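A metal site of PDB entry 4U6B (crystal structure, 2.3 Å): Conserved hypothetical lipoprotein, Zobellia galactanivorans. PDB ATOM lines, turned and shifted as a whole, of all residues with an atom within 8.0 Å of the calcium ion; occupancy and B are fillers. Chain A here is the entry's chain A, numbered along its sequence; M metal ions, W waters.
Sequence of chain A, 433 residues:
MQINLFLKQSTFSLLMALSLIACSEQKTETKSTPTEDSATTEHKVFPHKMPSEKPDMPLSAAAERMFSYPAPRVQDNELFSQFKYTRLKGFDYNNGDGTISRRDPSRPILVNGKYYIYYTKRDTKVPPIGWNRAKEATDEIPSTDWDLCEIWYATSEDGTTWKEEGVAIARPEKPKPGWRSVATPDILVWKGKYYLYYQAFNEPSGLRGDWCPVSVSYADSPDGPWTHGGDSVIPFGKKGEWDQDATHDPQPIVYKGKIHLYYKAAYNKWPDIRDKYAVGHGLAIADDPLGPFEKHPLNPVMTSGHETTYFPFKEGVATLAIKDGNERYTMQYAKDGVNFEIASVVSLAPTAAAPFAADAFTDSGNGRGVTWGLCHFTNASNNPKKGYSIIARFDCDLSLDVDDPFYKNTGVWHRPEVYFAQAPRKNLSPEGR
The backbone NH (N) of Asp 401 sits at hydrogen-bond distance from the side-chain hydroxyl (OG) of Ser 399 (3.2 Å).
N of Ser 399 lies within hydrogen-bond range of O of Val 370, 3.4 Å away.
O of Arg 368 is in hydrogen-bond range of OG of Ser 399, at 3.4 Å.
NZ of Lys 408 sits close to OD2 of Asp 397, 3.7 Å away.
N of Asp 404 sits close to OD2 of Asp 397, 3.1 Å away.
OG of Ser 81 is in hydrogen-bond range of N of Asp 397, at 2.8 Å.
The side-chain amino group of Lys 408 sits at hydrogen-bond distance from the backbone carbonyl oxygen of Asn 77, 3.1 Å away.
The side-chain amino group (NZ) of Lys 408 is in hydrogen-bond range of the backbone carbonyl oxygen (O) of Phe 80 (3.0 Å).
CA of Asp 403 touches the calcium ion, at 3.9 Å.
Lys 408 touches the calcium ion (NZ to CA, 3.997 Å).
Of the 20 residues printed, 6 come within 4 Å of the calcium ion.
Along chain A the residues within 4 Å of the calcium ion span positions 78 to 408.
The nearest printed residue that does not touch the calcium ion is Leu 400 (4.5 Å).
The calcium ion is bound by the backbone carbonyl oxygen (O) of Ser 399, the backbone carbonyl oxygen (O) of Val 402, water W2, the side-chain carboxylate (OE1) of Glu 78, the side-chain carboxylate (OD1) of Asp 397, water W3 and the side-chain carboxylate (OD2) of Asp 397.
Water W3 bridges the backbone carbonyl oxygen of Asp 397 (2.8 Å) and the backbone carbonyl oxygen of Glu 78 (2.8 Å).
Water W2 bridges NZ of Lys 408 and OD1 of Asp 403.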
ATOM      1  N   ASN A  77      22.101  -4.381  11.516  1.00  0.00           N
ATOM      2  CA  ASN A  77      23.328  -4.840  10.922  1.00  0.00           C
ATOM      3  C   ASN A  77      23.964  -5.796  11.942  1.00  0.00           C
ATOM      4  O   ASN A  77      24.000  -5.503  13.129  1.00  0.00           O
ATOM      5  CB  ASN A  77      24.176  -3.565  10.719  1.00  0.00           C
ATOM      6  CG  ASN A  77      25.558  -3.813  10.144  1.00  0.00           C
ATOM      7  OD1 ASN A  77      26.069  -4.937  10.114  1.00  0.00           O
ATOM      8  ND2 ASN A  77      26.177  -2.742   9.706  1.00  0.00           N
ATOM      9  N   GLU A  78      24.452  -6.952  11.501  1.00  0.00           N
ATOM     10  CA  GLU A  78      25.000  -7.908  12.465  1.00  0.00           C
ATOM     11  C   GLU A  78      26.369  -7.475  13.049  1.00  0.00           C
ATOM     12  O   GLU A  78      26.837  -8.032  14.046  1.00  0.00           O
ATOM     13  CB  GLU A  78      25.050  -9.300  11.866  1.00  0.00           C
ATOM     14  CG  GLU A  78      24.815 -10.421  12.878  1.00  0.00           C
ATOM     15  CD  GLU A  78      23.365 -10.646  13.273  1.00  0.00           C
ATOM     16  OE1 GLU A  78      23.040 -10.418  14.454  1.00  0.00           O
ATOM     17  OE2 GLU A  78      22.530 -11.072  12.436  1.00  0.00           O
ATOM     18  N   LEU A  79      26.973  -6.455  12.460  1.00  0.00           N
ATOM     19  CA  LEU A  79      28.229  -5.887  12.932  1.00  0.00           C
ATOM     20  C   LEU A  79      28.009  -4.518  13.508  1.00  0.00           C
ATOM     21  O   LEU A  79      28.930  -3.741  13.609  1.00  0.00           O
ATOM     22  CB  LEU A  79      29.268  -5.785  11.820  1.00  0.00           C
ATOM     23  CG  LEU A  79      30.400  -6.787  11.927  1.00  0.00           C
ATOM     24  CD1 LEU A  79      30.129  -7.839  13.013  1.00  0.00           C
ATOM     25  CD2 LEU A  79      30.656  -7.416  10.579  1.00  0.00           C
ATOM     26  N   PHE A  80      26.779  -4.198  13.878  1.00  0.00           N
ATOM     27  CA  PHE A  80      26.628  -2.935  14.578  1.00  0.00           C
ATOM     28  C   PHE A  80      26.261  -3.270  15.996  1.00  0.00           C
ATOM     29  O   PHE A  80      25.469  -4.196  16.215  1.00  0.00           O
ATOM     30  CB  PHE A  80      25.515  -2.091  14.005  1.00  0.00           C
ATOM     31  CG  PHE A  80      25.118  -0.995  14.921  1.00  0.00           C
ATOM     32  CD1 PHE A  80      25.822   0.212  14.923  1.00  0.00           C
ATOM     33  CD2 PHE A  80      24.086  -1.181  15.851  1.00  0.00           C
ATOM     34  CE1 PHE A  80      25.471   1.245  15.805  1.00  0.00           C
ATOM     35  CE2 PHE A  80      23.762  -0.167  16.741  1.00  0.00           C
ATOM     36  CZ  PHE A  80      24.458   1.049  16.724  1.00  0.00           C
ATOM     37  N   SER A  81      26.803  -2.507  16.954  1.00  0.00           N
ATOM     38  CA  SER A  81      26.472  -2.755  18.383  1.00  0.00           C
ATOM     39  C   SER A  81      26.854  -1.607  19.238  1.00  0.00           C
ATOM     40  O   SER A  81      27.716  -0.797  18.892  1.00  0.00           O
ATOM     41  CB  SER A  81      27.143  -4.044  18.933  1.00  0.00           C
ATOM     42  OG  SER A  81      26.720  -4.391  20.263  1.00  0.00           O
ATOM     43  N   PHE A 313      34.962 -13.963  11.220  1.00  0.00           N
ATOM     44  CA  PHE A 313      33.560 -13.662  11.016  1.00  0.00           C
ATOM     45  C   PHE A 313      33.058 -14.187   9.652  1.00  0.00           C
ATOM     46  O   PHE A 313      33.501 -13.691   8.585  1.00  0.00           O
ATOM     47  CB  PHE A 313      33.343 -12.176  11.094  1.00  0.00           C
ATOM     48  CG  PHE A 313      31.916 -11.793  11.324  1.00  0.00           C
ATOM     49  CD1 PHE A 313      31.289 -12.119  12.513  1.00  0.00           C
ATOM     50  CD2 PHE A 313      31.226 -11.066  10.370  1.00  0.00           C
ATOM     51  CE1 PHE A 313      29.978 -11.726  12.738  1.00  0.00           C
ATOM     52  CE2 PHE A 313      29.900 -10.670  10.586  1.00  0.00           C
ATOM     53  CZ  PHE A 313      29.280 -11.004  11.775  1.00  0.00           C
ATOM     54  N   ARG A 368      31.551 -16.966  14.159  1.00  0.00           N
ATOM     55  CA  ARG A 368      30.234 -16.622  14.743  1.00  0.00           C
ATOM     56  C   ARG A 368      30.078 -15.220  15.347  1.00  0.00           C
ATOM     57  O   ARG A 368      28.948 -14.799  15.665  1.00  0.00           O
ATOM     58  CB  ARG A 368      29.827 -17.694  15.734  1.00  0.00           C
ATOM     59  CG  ARG A 368      29.740 -19.086  15.121  1.00  0.00           C
ATOM     60  CD  ARG A 368      28.314 -19.369  14.653  1.00  0.00           C
ATOM     61  NE  ARG A 368      28.075 -19.104  13.238  1.00  0.00           N
ATOM     62  CZ  ARG A 368      26.889 -18.873  12.683  1.00  0.00           C
ATOM     63  NH1 ARG A 368      26.813 -18.657  11.390  1.00  0.00           N
ATOM     64  NH2 ARG A 368      25.792 -18.823  13.421  1.00  0.00           N
ATOM     65  N   VAL A 370      31.118 -12.141  18.377  1.00  0.00           N
ATOM     66  CA  VAL A 370      31.470 -12.002  19.807  1.00  0.00           C
ATOM     67  C   VAL A 370      30.403 -11.264  20.592  1.00  0.00           C
ATOM     68  O   VAL A 370      29.678 -10.409  20.013  1.00  0.00           O
ATOM     69  CB  VAL A 370      32.829 -11.280  19.979  1.00  0.00           C
ATOM     70  CG1 VAL A 370      33.883 -12.016  19.205  1.00  0.00           C
ATOM     71  CG2 VAL A 370      32.767  -9.837  19.509  1.00  0.00           C
ATOM     72  N   THR A 371      30.339 -11.558  21.908  1.00  0.00           N
ATOM     73  CA  THR A 371      29.442 -10.828  22.836  1.00  0.00           C
ATOM     74  C   THR A 371      30.175 -10.200  24.043  1.00  0.00           C
ATOM     75  O   THR A 371      29.650  -9.292  24.669  1.00  0.00           O
ATOM     76  CB  THR A 371      28.272 -11.701  23.393  1.00  0.00           C
ATOM     77  OG1 THR A 371      28.791 -12.847  24.072  1.00  0.00           O
ATOM     78  CG2 THR A 371      27.394 -12.214  22.235  1.00  0.00           C
ATOM     79  N   CYS A 396      28.814  -6.907  24.295  1.00  0.00           N
ATOM     80  CA  CYS A 396      28.227  -6.277  23.115  1.00  0.00           C
ATOM     81  C   CYS A 396      27.381  -7.363  22.411  1.00  0.00           C
ATOM     82  O   CYS A 396      27.266  -8.493  22.947  1.00  0.00           O
ATOM     83  CB  CYS A 396      29.343  -5.732  22.181  1.00  0.00           C
ATOM     84  SG  CYS A 396      30.366  -7.113  21.672  1.00  0.00           S
ATOM     85  N   ASP A 397      26.779  -7.032  21.263  1.00  0.00           N
ATOM     86  CA  ASP A 397      26.235  -8.061  20.399  1.00  0.00           C
ATOM     87  C   ASP A 397      26.835  -7.892  19.006  1.00  0.00           C
ATOM     88  O   ASP A 397      26.328  -7.088  18.197  1.00  0.00           O
ATOM     89  CB  ASP A 397      24.690  -8.033  20.344  1.00  0.00           C
ATOM     90  CG  ASP A 397      24.132  -9.014  19.301  1.00  0.00           C
ATOM     91  OD1 ASP A 397      24.859  -9.987  18.935  1.00  0.00           O
ATOM     92  OD2 ASP A 397      22.993  -8.827  18.832  1.00  0.00           O
ATOM     93  N   LEU A 398      27.952  -8.563  18.772  1.00  0.00           N
ATOM     94  CA  LEU A 398      28.550  -8.609  17.444  1.00  0.00           C
ATOM     95  C   LEU A 398      28.562 -10.092  17.085  1.00  0.00           C
ATOM     96  O   LEU A 398      29.536 -10.613  16.510  1.00  0.00           O
ATOM     97  CB  LEU A 398      29.965  -8.000  17.491  1.00  0.00           C
ATOM     98  CG  LEU A 398      30.021  -6.506  17.877  1.00  0.00           C
ATOM     99  CD1 LEU A 398      31.435  -6.039  18.221  1.00  0.00           C
ATOM    100  CD2 LEU A 398      29.430  -5.648  16.753  1.00  0.00           C
ATOM    101  N   SER A 399      27.480 -10.769  17.493  1.00  0.00           N
ATOM    102  CA  SER A 399      27.306 -12.198  17.303  1.00  0.00           C
ATOM    103  C   SER A 399      26.204 -12.536  16.289  1.00  0.00           C
ATOM    104  O   SER A 399      25.103 -11.928  16.291  1.00  0.00           O
ATOM    105  CB  SER A 399      26.899 -12.854  18.605  1.00  0.00           C
ATOM    106  OG  SER A 399      27.086 -14.249  18.511  1.00  0.00           O
ATOM    107  N   LEU A 400      26.496 -13.554  15.470  1.00  0.00           N
ATOM    108  CA  LEU A 400      25.494 -14.161  14.585  1.00  0.00           C
ATOM    109  C   LEU A 400      24.555 -15.088  15.361  1.00  0.00           C
ATOM    110  O   LEU A 400      23.406 -15.274  14.984  1.00  0.00           O
ATOM    111  CB  LEU A 400      26.149 -14.906  13.427  1.00  0.00           C
ATOM    112  CG  LEU A 400      27.042 -14.090  12.479  1.00  0.00           C
ATOM    113  CD1 LEU A 400      27.587 -15.005  11.382  1.00  0.00           C
ATOM    114  CD2 LEU A 400      26.310 -12.904  11.880  1.00  0.00           C
ATOM    115  N   ASP A 401      25.036 -15.643  16.468  1.00  0.00           N
ATOM    116  CA  ASP A 401      24.275 -16.577  17.257  1.00  0.00           C
ATOM    117  C   ASP A 401      23.470 -15.951  18.368  1.00  0.00           C
ATOM    118  O   ASP A 401      22.907 -16.680  19.173  1.00  0.00           O
ATOM    119  CB  ASP A 401      25.193 -17.627  17.862  1.00  0.00           C
ATOM    120  CG  ASP A 401      25.758 -18.569  16.823  1.00  0.00           C
ATOM    121  OD1 ASP A 401      25.093 -18.860  15.802  1.00  0.00           O
ATOM    122  OD2 ASP A 401      26.884 -19.035  17.034  1.00  0.00           O
ATOM    123  N   VAL A 402      23.401 -14.617  18.435  1.00  0.00           N
ATOM    124  CA  VAL A 402      22.652 -13.948  19.515  1.00  0.00           C
ATOM    125  C   VAL A 402      22.136 -12.703  18.888  1.00  0.00           C
ATOM    126  O   VAL A 402      22.835 -12.109  18.073  1.00  0.00           O
ATOM    127  CB  VAL A 402      23.582 -13.421  20.671  1.00  0.00           C
ATOM    128  CG1 VAL A 402      22.810 -12.555  21.687  1.00  0.00           C
ATOM    129  CG2 VAL A 402      24.343 -14.542  21.371  1.00  0.00           C
ATOM    130  N   ASP A 403      20.965 -12.257  19.329  1.00  0.00           N
ATOM    131  CA  ASP A 403      20.398 -10.986  18.905  1.00  0.00           C
ATOM    132  C   ASP A 403      19.785 -10.263  20.121  1.00  0.00           C
ATOM    133  O   ASP A 403      18.719 -10.636  20.626  1.00  0.00           O
ATOM    134  CB  ASP A 403      19.371 -11.212  17.751  1.00  0.00           C
ATOM    135  CG  ASP A 403      18.774  -9.920  17.229  1.00  0.00           C
ATOM    136  OD1 ASP A 403      19.489  -8.904  17.035  1.00  0.00           O
ATOM    137  OD2 ASP A 403      17.545  -9.924  16.999  1.00  0.00           O
ATOM    138  N   ASP A 404      20.474  -9.242  20.609  1.00  0.00           N
ATOM    139  CA  ASP A 404      20.095  -8.649  21.892  1.00  0.00           C
ATOM    140  C   ASP A 404      19.755  -7.225  21.683  1.00  0.00           C
ATOM    141  O   ASP A 404      20.640  -6.387  21.577  1.00  0.00           O
ATOM    142  CB  ASP A 404      21.206  -8.814  22.922  1.00  0.00           C
ATOM    143  CG  ASP A 404      20.782  -8.410  24.342  1.00  0.00           C
ATOM    144  OD1 ASP A 404      19.877  -7.556  24.532  1.00  0.00           O
ATOM    145  OD2 ASP A 404      21.413  -8.956  25.273  1.00  0.00           O
ATOM    146  N   PRO A 405      18.453  -6.920  21.625  1.00  0.00           N
ATOM    147  CA  PRO A 405      18.010  -5.543  21.369  1.00  0.00           C
ATOM    148  C   PRO A 405      18.593  -4.529  22.362  1.00  0.00           C
ATOM    149  O   PRO A 405      18.595  -3.322  22.072  1.00  0.00           O
ATOM    150  CB  PRO A 405      16.478  -5.629  21.511  1.00  0.00           C
ATOM    151  CG  PRO A 405      16.204  -6.945  22.189  1.00  0.00           C
ATOM    152  CD  PRO A 405      17.319  -7.855  21.778  1.00  0.00           C
ATOM    153  N   LYS A 408      21.446  -2.668  20.799  1.00  0.00           N
ATOM    154  CA  LYS A 408      21.169  -2.434  19.424  1.00  0.00           C
ATOM    155  C   LYS A 408      20.513  -1.068  19.237  1.00  0.00           C
ATOM    156  O   LYS A 408      20.231  -0.666  18.128  1.00  0.00           O
ATOM    157  CB  LYS A 408      20.385  -3.633  18.886  1.00  0.00           C
ATOM    158  CG  LYS A 408      20.948  -4.189  17.586  1.00  0.00           C
ATOM    159  CD  LYS A 408      22.050  -5.236  17.673  1.00  0.00           C
ATOM    160  CE  LYS A 408      22.688  -5.338  16.302  1.00  0.00           C
ATOM    161  NZ  LYS A 408      23.570  -6.502  16.055  1.00  0.00           N
HETATM  162 CA    CA M   1      23.588 -10.434  16.774  1.00  0.00          CA
HETATM  163  O   HOH W   1      21.728 -12.876  15.587  1.00  0.00           O
HETATM  164  O   HOH W   2      22.062  -8.723  16.131  1.00  0.00           O
HETATM  165  O   HOH W   3      24.957  -8.344  16.129  1.00  0.00           O
